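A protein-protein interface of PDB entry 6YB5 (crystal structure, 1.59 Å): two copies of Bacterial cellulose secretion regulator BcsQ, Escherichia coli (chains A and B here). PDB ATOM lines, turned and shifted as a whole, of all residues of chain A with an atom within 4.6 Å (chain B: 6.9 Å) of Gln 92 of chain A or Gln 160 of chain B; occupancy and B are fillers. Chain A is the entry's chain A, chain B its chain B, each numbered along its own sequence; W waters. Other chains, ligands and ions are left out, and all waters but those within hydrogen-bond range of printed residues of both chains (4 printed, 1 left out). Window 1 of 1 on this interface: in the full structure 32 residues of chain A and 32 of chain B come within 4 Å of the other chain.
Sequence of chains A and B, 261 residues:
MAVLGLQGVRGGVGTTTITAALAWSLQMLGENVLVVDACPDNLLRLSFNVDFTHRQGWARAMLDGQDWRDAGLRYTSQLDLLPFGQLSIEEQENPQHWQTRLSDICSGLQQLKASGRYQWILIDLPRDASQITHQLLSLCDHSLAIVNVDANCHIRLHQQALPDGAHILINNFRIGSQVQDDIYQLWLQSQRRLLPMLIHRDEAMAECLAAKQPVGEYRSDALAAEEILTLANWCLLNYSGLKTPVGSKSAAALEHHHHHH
O of Gln 159 of chain B lies within hydrogen-bond range of NE2 of Gln 92 of chain A (2.8 Å). O of Glu 93 of chain A sits at hydrogen-bond distance from NE2 of His 134 of chain B (3.0 Å).
NE2 of Gln 92 of chain A sits at hydrogen-bond distance from O of Leu 87 of chain A, 3.2 Å away. The backbone carbonyl oxygen (O) of Val 9 of chain B lies within hydrogen-bond range of the side-chain amide nitrogen (NE2) of Gln 160 of chain B (2.9 Å). The side-chain amide nitrogen (NE2) of Gln 160 of chain B sits close to the guanidinium group (NE) of Arg 127 of chain B. NH1 of Arg 156 of chain B is in hydrogen-bond range of OE1 of Gln 160 of chain B (2.9 Å).
Among the printed residues, pairs that only touch across the chains: Gln 92 of chain A with Gln 160 of chain B, Glu 93 of chain A with Ala 129 of chain B, Ile 89 of chain A with Gln 159 of chain B, Gln 92 of chain A with Ala 129 of chain B, Pro 95 of chain A with Ala 129 of chain B, Ile 89 of chain A with Ala 161 of chain B and Ile 89 of chain A with Gln 160 of chain B.
Of chain B, only Ala 129, Gln 159 and Gln 160 come within 4 Å of Gln 92 of chain A. Of the printed residues of chain B, Glu 93 of chain A touches Ala 129 (3.5 Å) and His 134 (3.0 Å). Val 9 of chain B touches none of the printed residues of chain A. Arg 127 of chain B touches none of the printed residues of chain A. Of the printed residues of chain A, Ala 129 of chain B touches Gln 92, Glu 93 and Pro 95. Printed residues of chain A within 4 Å of His 134 of chain B: Glu 93 (3.0 Å). Of the printed residues of chain A, Gln 159 of chain B touches Ile 89 (3.5 Å) and Gln 92 (2.8 Å). Of chain A, only Ile 89 and Gln 92 come within 4 Å of Gln 160 of chain B. Of the printed residues of chain A, Ala 161 of chain B touches Ile 89.
Printed residues of chain B that touch a printed residue of chain A: Ala 129, His 134, Gln 159, Gln 160 and Ala 161. Hydrophobic or aromatic side chains of chain B that line the printed part of chain A: Ala 129 and His 134. Among the printed residues, no Asp or Glu carboxylate lies within 4 Å of a Lys or Arg side-chain nitrogen of the other chain.
No position is printed for both chains.
Water W4 lies within hydrogen-bond range of OE2 of Glu 93 of chain A (2.4 Å), OE1 of Gln 92 of chain A (2.8 Å) and N of Ala 161 of chain B (2.9 Å). Water W1 lies within hydrogen-bond range of the guanidinium group of Arg 127 of chain B, the backbone carbonyl oxygen of Ala 161 of chain B and the side-chain carboxylate of Glu 93 of chain A. Water W2 lies within hydrogen-bond range of O of Gln 92 of chain A (3.0 Å) and NH2 of Arg 127 of chain B (3.3 Å). Water W3 lies within hydrogen-bond range of NE2 of Gln 159 of chain B (3.1 Å) and NE2 of Gln 92 of chain A (3.2 Å).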
ATOM      1  N   LEU A  87      23.764  19.305  26.994  1.00  0.00           N
ATOM      2  CA  LEU A  87      25.062  18.636  27.106  1.00  0.00           C
ATOM      3  C   LEU A  87      25.794  18.599  25.764  1.00  0.00           C
ATOM      4  O   LEU A  87      25.172  18.434  24.711  1.00  0.00           O
ATOM      5  CB  LEU A  87      24.885  17.193  27.587  1.00  0.00           C
ATOM      6  CG  LEU A  87      24.326  16.925  28.978  1.00  0.00           C
ATOM      7  CD1 LEU A  87      24.180  15.433  29.185  1.00  0.00           C
ATOM      8  CD2 LEU A  87      25.242  17.528  30.022  1.00  0.00           C
ATOM      9  N   SER A  88      27.124  18.716  25.812  1.00  0.00           N
ATOM     10  CA  SER A  88      27.930  18.508  24.613  1.00  0.00           C
ATOM     11  C   SER A  88      27.876  17.041  24.190  1.00  0.00           C
ATOM     12  O   SER A  88      27.474  16.163  24.955  1.00  0.00           O
ATOM     13  CB  SER A  88      29.382  18.905  24.860  1.00  0.00           C
ATOM     14  OG  SER A  88      30.018  17.945  25.691  1.00  0.00           O
ATOM     15  N   ILE A  89      28.301  16.778  22.951  1.00  0.00           N
ATOM     16  CA  ILE A  89      28.322  15.397  22.470  1.00  0.00           C
ATOM     17  C   ILE A  89      29.239  14.544  23.340  1.00  0.00           C
ATOM     18  O   ILE A  89      28.923  13.392  23.653  1.00  0.00           O
ATOM     19  CB  ILE A  89      28.732  15.346  20.985  1.00  0.00           C
ATOM     20  CG1 ILE A  89      27.658  16.005  20.115  1.00  0.00           C
ATOM     21  CG2 ILE A  89      28.953  13.905  20.536  1.00  0.00           C
ATOM     22  CD1 ILE A  89      26.329  15.263  20.105  1.00  0.00           C
ATOM     23  N   GLU A  90      30.367  15.107  23.784  1.00  0.00           N
ATOM     24  CA  GLU A  90      31.279  14.329  24.619  1.00  0.00           C
ATOM     25  C   GLU A  90      30.653  13.997  25.967  1.00  0.00           C
ATOM     26  O   GLU A  90      30.795  12.871  26.462  1.00  0.00           O
ATOM     27  CB  GLU A  90      32.598  15.074  24.799  1.00  0.00           C
ATOM     28  CG  GLU A  90      33.416  15.158  23.519  1.00  0.00           C
ATOM     29  CD  GLU A  90      33.700  13.789  22.916  1.00  0.00           C
ATOM     30  OE1 GLU A  90      34.116  12.884  23.672  1.00  0.00           O
ATOM     31  OE2 GLU A  90      33.499  13.621  21.691  1.00  0.00           O
ATOM     32  N   GLU A  91      29.952  14.958  26.573  1.00  0.00           N
ATOM     33  CA  GLU A  91      29.219  14.669  27.800  1.00  0.00           C
ATOM     34  C   GLU A  91      28.132  13.632  27.550  1.00  0.00           C
ATOM     35  O   GLU A  91      27.930  12.724  28.367  1.00  0.00           O
ATOM     36  CB  GLU A  91      28.618  15.960  28.364  1.00  0.00           C
ATOM     37  CG  GLU A  91      29.661  16.937  28.922  1.00  0.00           C
ATOM     38  CD  GLU A  91      29.095  18.315  29.216  1.00  0.00           C
ATOM     39  OE1 GLU A  91      28.256  18.809  28.432  1.00  0.00           O
ATOM     40  OE2 GLU A  91      29.488  18.906  30.244  1.00  0.00           O
ATOM     41  N   GLN A  92      27.434  13.734  26.412  1.00  0.00           N
ATOM     42  CA  GLN A  92      26.400  12.755  26.077  1.00  0.00           C
ATOM     43  C   GLN A  92      26.969  11.350  25.936  1.00  0.00           C
ATOM     44  O   GLN A  92      26.327  10.371  26.334  1.00  0.00           O
ATOM     45  CB  GLN A  92      25.709  13.133  24.769  1.00  0.00           C
ATOM     46  CG  GLN A  92      24.857  14.364  24.814  1.00  0.00           C
ATOM     47  CD  GLN A  92      24.239  14.641  23.447  1.00  0.00           C
ATOM     48  OE1 GLN A  92      23.870  13.709  22.723  1.00  0.00           O
ATOM     49  NE2 GLN A  92      24.157  15.912  23.074  1.00  0.00           N
ATOM     50  N   GLU A  93      28.141  11.224  25.318  1.00  0.00           N
ATOM     51  CA  GLU A  93      28.718   9.919  25.031  1.00  0.00           C
ATOM     52  C   GLU A  93      29.498   9.339  26.201  1.00  0.00           C
ATOM     53  O   GLU A  93      29.865   8.162  26.156  1.00  0.00           O
ATOM     54  CB  GLU A  93      29.630  10.011  23.804  1.00  0.00           C
ATOM     55  CG  GLU A  93      28.920  10.509  22.545  1.00  0.00           C
ATOM     56  CD  GLU A  93      27.790   9.596  22.104  1.00  0.00           C
ATOM     57  OE1 GLU A  93      27.902   8.367  22.301  1.00  0.00           O
ATOM     58  OE2 GLU A  93      26.785  10.106  21.565  1.00  0.00           O
ATOM     59  N   ASN A  94      29.759  10.121  27.245  1.00  0.00           N
ATOM     60  CA  ASN A  94      30.492   9.640  28.418  1.00  0.00           C
ATOM     61  C   ASN A  94      29.762  10.047  29.691  1.00  0.00           C
ATOM     62  O   ASN A  94      30.277  10.823  30.501  1.00  0.00           O
ATOM     63  CB  ASN A  94      31.924  10.173  28.406  1.00  0.00           C
ATOM     64  CG  ASN A  94      32.678   9.785  27.150  1.00  0.00           C
ATOM     65  OD1 ASN A  94      33.156   8.657  27.024  1.00  0.00           O
ATOM     66  ND2 ASN A  94      32.789  10.718  26.212  1.00  0.00           N
ATOM     67  N   PRO A  95      28.544   9.536  29.905  1.00  0.00           N
ATOM     68  CA  PRO A  95      27.750  10.010  31.049  1.00  0.00           C
ATOM     69  C   PRO A  95      28.326   9.621  32.397  1.00  0.00           C
ATOM     70  O   PRO A  95      28.023  10.289  33.394  1.00  0.00           O
ATOM     71  CB  PRO A  95      26.377   9.362  30.817  1.00  0.00           C
ATOM     72  CG  PRO A  95      26.672   8.144  30.049  1.00  0.00           C
ATOM     73  CD  PRO A  95      27.821   8.510  29.130  1.00  0.00           C
ATOM     74  N   GLN B   7      20.554   0.629  15.531  1.00  0.00           N
ATOM     75  CA  GLN B   7      20.466   1.341  16.800  1.00  0.00           C
ATOM     76  C   GLN B   7      19.382   2.399  16.708  1.00  0.00           C
ATOM     77  O   GLN B   7      19.408   3.234  15.803  1.00  0.00           O
ATOM     78  CB  GLN B   7      21.810   1.998  17.138  1.00  0.00           C
ATOM     79  CG  GLN B   7      21.840   2.657  18.509  1.00  0.00           C
ATOM     80  CD  GLN B   7      23.101   3.457  18.746  1.00  0.00           C
ATOM     81  OE1 GLN B   7      23.424   4.375  17.991  1.00  0.00           O
ATOM     82  NE2 GLN B   7      23.828   3.109  19.802  1.00  0.00           N
ATOM     83  N   GLY B   8      18.439   2.374  17.643  1.00  0.00           N
ATOM     84  CA  GLY B   8      17.400   3.398  17.646  1.00  0.00           C
ATOM     85  C   GLY B   8      17.938   4.753  18.081  1.00  0.00           C
ATOM     86  O   GLY B   8      18.817   4.856  18.946  1.00  0.00           O
ATOM     87  N   VAL B   9      17.405   5.808  17.456  1.00  0.00           N
ATOM     88  CA  VAL B   9      17.707   7.171  17.879  1.00  0.00           C
ATOM     89  C   VAL B   9      17.106   7.447  19.257  1.00  0.00           C
ATOM     90  O   VAL B   9      17.611   8.293  20.006  1.00  0.00           O
ATOM     91  CB  VAL B   9      17.223   8.143  16.779  1.00  0.00           C
ATOM     92  CG1 VAL B   9      17.195   9.575  17.264  1.00  0.00           C
ATOM     93  CG2 VAL B   9      18.138   8.035  15.559  1.00  0.00           C
ATOM     94  N   ARG B  10      16.065   6.707  19.630  1.00  0.00           N
ATOM     95  CA  ARG B  10      15.568   6.687  20.998  1.00  0.00           C
ATOM     96  C   ARG B  10      14.978   5.309  21.239  1.00  0.00           C
ATOM     97  O   ARG B  10      14.883   4.490  20.332  1.00  0.00           O
ATOM     98  CB  ARG B  10      14.545   7.789  21.264  1.00  0.00           C
ATOM     99  CG  ARG B  10      13.269   7.598  20.536  1.00  0.00           C
ATOM    100  CD  ARG B  10      12.075   8.158  21.327  1.00  0.00           C
ATOM    101  NE  ARG B  10      10.857   7.717  20.662  1.00  0.00           N
ATOM    102  CZ  ARG B  10      10.225   8.403  19.718  1.00  0.00           C
ATOM    103  NH1 ARG B  10      10.672   9.592  19.348  1.00  0.00           N
ATOM    104  NH2 ARG B  10       9.134   7.902  19.152  1.00  0.00           N
ATOM    105  N   ARG B 127      21.237   2.371  22.836  1.00  0.00           N
ATOM    106  CA  ARG B 127      21.856   3.685  22.762  1.00  0.00           C
ATOM    107  C   ARG B 127      22.020   4.223  24.179  1.00  0.00           C
ATOM    108  O   ARG B 127      21.470   5.265  24.551  1.00  0.00           O
ATOM    109  CB  ARG B 127      21.031   4.625  21.894  1.00  0.00           C
ATOM    110  CG  ARG B 127      21.878   5.766  21.369  1.00  0.00           C
ATOM    111  CD  ARG B 127      21.072   6.820  20.660  1.00  0.00           C
ATOM    112  NE  ARG B 127      21.755   8.097  20.812  1.00  0.00           N
ATOM    113  CZ  ARG B 127      21.617   8.888  21.872  1.00  0.00           C
ATOM    114  NH1 ARG B 127      20.807   8.544  22.863  1.00  0.00           N
ATOM    115  NH2 ARG B 127      22.286  10.027  21.935  1.00  0.00           N
ATOM    116  N   ASP B 128      22.813   3.512  24.970  1.00  0.00           N
ATOM    117  CA  ASP B 128      23.010   3.818  26.377  1.00  0.00           C
ATOM    118  C   ASP B 128      24.393   4.399  26.673  1.00  0.00           C
ATOM    119  O   ASP B 128      24.742   4.578  27.848  1.00  0.00           O
ATOM    120  CB  ASP B 128      22.762   2.564  27.229  1.00  0.00           C
ATOM    121  CG  ASP B 128      23.633   1.378  26.825  1.00  0.00           C
ATOM    122  OD1 ASP B 128      24.571   1.540  26.001  1.00  0.00           O
ATOM    123  OD2 ASP B 128      23.385   0.272  27.360  1.00  0.00           O
ATOM    124  N   ALA B 129      25.184   4.694  25.641  1.00  0.00           N
ATOM    125  CA  ALA B 129      26.490   5.351  25.775  1.00  0.00           C
ATOM    126  C   ALA B 129      27.458   4.576  26.668  1.00  0.00           C
ATOM    127  O   ALA B 129      28.366   5.160  27.259  1.00  0.00           O
ATOM    128  CB  ALA B 129      26.342   6.790  26.280  1.00  0.00           C
ATOM    129  N   HIS B 134      29.819   1.333  22.678  1.00  0.00           N
ATOM    130  CA  HIS B 134      30.724   2.046  21.779  1.00  0.00           C
ATOM    131  C   HIS B 134      31.650   1.076  21.061  1.00  0.00           C
ATOM    132  O   HIS B 134      31.906   1.223  19.859  1.00  0.00           O
ATOM    133  CB  HIS B 134      31.546   3.074  22.554  1.00  0.00           C
ATOM    134  CG  HIS B 134      30.752   4.238  23.063  1.00  0.00           C
ATOM    135  ND1 HIS B 134      29.736   4.823  22.338  1.00  0.00           N
ATOM    136  CD2 HIS B 134      30.826   4.926  24.227  1.00  0.00           C
ATOM    137  CE1 HIS B 134      29.218   5.820  23.032  1.00  0.00           C
ATOM    138  NE2 HIS B 134      29.862   5.905  24.182  1.00  0.00           N
ATOM    139  N   ASN B 152       9.860  14.340  18.596  1.00  0.00           N
ATOM    140  CA  ASN B 152      10.959  13.915  19.452  1.00  0.00           C
ATOM    141  C   ASN B 152      12.167  13.494  18.614  1.00  0.00           C
ATOM    142  O   ASN B 152      13.284  13.975  18.837  1.00  0.00           O
ATOM    143  CB  ASN B 152      10.439  12.792  20.371  1.00  0.00           C
ATOM    144  CG  ASN B 152      11.515  12.112  21.213  1.00  0.00           C
ATOM    145  OD1 ASN B 152      12.597  11.794  20.748  1.00  0.00           O
ATOM    146  ND2 ASN B 152      11.161  11.804  22.465  1.00  0.00           N
ATOM    147  N   ILE B 155      13.847  16.538  16.948  1.00  0.00           N
ATOM    148  CA  ILE B 155      14.740  17.288  17.828  1.00  0.00           C
ATOM    149  C   ILE B 155      16.046  16.531  18.032  1.00  0.00           C
ATOM    150  O   ILE B 155      17.140  17.113  18.008  1.00  0.00           O
ATOM    151  CB  ILE B 155      14.048  17.557  19.179  1.00  0.00           C
ATOM    152  CG1 ILE B 155      12.806  18.428  19.003  1.00  0.00           C
ATOM    153  CG2 ILE B 155      15.033  18.168  20.155  1.00  0.00           C
ATOM    154  CD1 ILE B 155      11.731  18.145  20.083  1.00  0.00           C
ATOM    155  N   ARG B 156      15.947  15.221  18.276  1.00  0.00           N
ATOM    156  CA  ARG B 156      17.141  14.427  18.554  1.00  0.00           C
ATOM    157  C   ARG B 156      18.129  14.481  17.400  1.00  0.00           C
ATOM    158  O   ARG B 156      19.344  14.514  17.623  1.00  0.00           O
ATOM    159  CB  ARG B 156      16.756  12.982  18.855  1.00  0.00           C
ATOM    160  CG  ARG B 156      16.102  12.806  20.215  1.00  0.00           C
ATOM    161  CD  ARG B 156      15.766  11.331  20.418  1.00  0.00           C
ATOM    162  NE  ARG B 156      15.250  11.074  21.758  1.00  0.00           N
ATOM    163  CZ  ARG B 156      16.008  10.742  22.791  1.00  0.00           C
ATOM    164  NH1 ARG B 156      17.324  10.640  22.638  1.00  0.00           N
ATOM    165  NH2 ARG B 156      15.450  10.522  23.984  1.00  0.00           N
ATOM    166  N   LEU B 157      17.630  14.525  16.159  1.00  0.00           N
ATOM    167  CA  LEU B 157      18.545  14.569  15.023  1.00  0.00           C
ATOM    168  C   LEU B 157      19.390  15.843  15.003  1.00  0.00           C
ATOM    169  O   LEU B 157      20.410  15.888  14.299  1.00  0.00           O
ATOM    170  CB  LEU B 157      17.757  14.427  13.721  1.00  0.00           C
ATOM    171  CG  LEU B 157      17.137  13.060  13.426  1.00  0.00           C
ATOM    172  CD1 LEU B 157      16.215  13.145  12.211  1.00  0.00           C
ATOM    173  CD2 LEU B 157      18.212  11.994  13.223  1.00  0.00           C
ATOM    174  N   HIS B 158      18.991  16.880  15.745  1.00  0.00           N
ATOM    175  CA  HIS B 158      19.739  18.132  15.823  1.00  0.00           C
ATOM    176  C   HIS B 158      20.608  18.252  17.066  1.00  0.00           C
ATOM    177  O   HIS B 158      21.248  19.292  17.251  1.00  0.00           O
ATOM    178  CB  HIS B 158      18.795  19.335  15.795  1.00  0.00           C
ATOM    179  CG  HIS B 158      18.035  19.478  14.521  1.00  0.00           C
ATOM    180  ND1 HIS B 158      16.890  18.758  14.252  1.00  0.00           N
ATOM    181  CD2 HIS B 158      18.247  20.268  13.440  1.00  0.00           C
ATOM    182  CE1 HIS B 158      16.436  19.090  13.055  1.00  0.00           C
ATOM    183  NE2 HIS B 158      17.243  20.004  12.541  1.00  0.00           N
ATOM    184  N   GLN B 159      20.630  17.249  17.939  1.00  0.00           N
ATOM    185  CA  GLN B 159      21.417  17.402  19.156  1.00  0.00           C
ATOM    186  C   GLN B 159      22.184  16.168  19.588  1.00  0.00           C
ATOM    187  O   GLN B 159      22.959  16.272  20.543  1.00  0.00           O
ATOM    188  CB  GLN B 159      20.533  17.858  20.329  1.00  0.00           C
ATOM    189  CG  GLN B 159      19.411  16.905  20.681  1.00  0.00           C
ATOM    190  CD  GLN B 159      18.725  17.328  21.956  1.00  0.00           C
ATOM    191  OE1 GLN B 159      18.655  18.525  22.268  1.00  0.00           O
ATOM    192  NE2 GLN B 159      18.239  16.353  22.718  1.00  0.00           N
ATOM    193  N   GLN B 160      22.031  15.024  18.937  1.00  0.00           N
ATOM    194  CA  GLN B 160      22.805  13.851  19.312  1.00  0.00           C
ATOM    195  C   GLN B 160      23.499  13.287  18.082  1.00  0.00           C
ATOM    196  O   GLN B 160      23.118  13.563  16.942  1.00  0.00           O
ATOM    197  CB  GLN B 160      21.925  12.782  19.998  1.00  0.00           C
ATOM    198  CG  GLN B 160      20.996  12.062  19.070  1.00  0.00           C
ATOM    199  CD  GLN B 160      19.974  11.197  19.802  1.00  0.00           C
ATOM    200  OE1 GLN B 160      19.294  11.648  20.735  1.00  0.00           O
ATOM    201  NE2 GLN B 160      19.832   9.961  19.349  1.00  0.00           N
ATOM    202  N   ALA B 161      24.559  12.531  18.327  1.00  0.00           N
ATOM    203  CA  ALA B 161      25.308  11.922  17.240  1.00  0.00           C
ATOM    204  C   ALA B 161      24.591  10.686  16.705  1.00  0.00           C
ATOM    205  O   ALA B 161      23.995   9.912  17.459  1.00  0.00           O
ATOM    206  CB  ALA B 161      26.713  11.535  17.706  1.00  0.00           C
ATOM    207  N   LEU B 162      24.639  10.524  15.400  1.00  0.00           N
ATOM    208  CA  LEU B 162      24.307   9.263  14.752  1.00  0.00           C
ATOM    209  C   LEU B 162      25.571   8.430  14.609  1.00  0.00           C
ATOM    210  O   LEU B 162      26.681   8.970  14.627  1.00  0.00           O
ATOM    211  CB  LEU B 162      23.708   9.521  13.367  1.00  0.00           C
ATOM    212  CG  LEU B 162      22.361  10.236  13.245  1.00  0.00           C
ATOM    213  CD1 LEU B 162      22.134  10.690  11.810  1.00  0.00           C
ATOM    214  CD2 LEU B 162      21.240   9.337  13.698  1.00  0.00           C
HETATM  215  O   HOH W   1      23.994   9.073  20.087  1.00  0.00           O
HETATM  216  O   HOH W   2      24.163   9.317  24.596  1.00  0.00           O
HETATM  217  O   HOH W   3      21.062  15.230  23.349  1.00  0.00           O
HETATM  218  O   HOH W   4      25.229  11.911  21.030  1.00  0.00           O
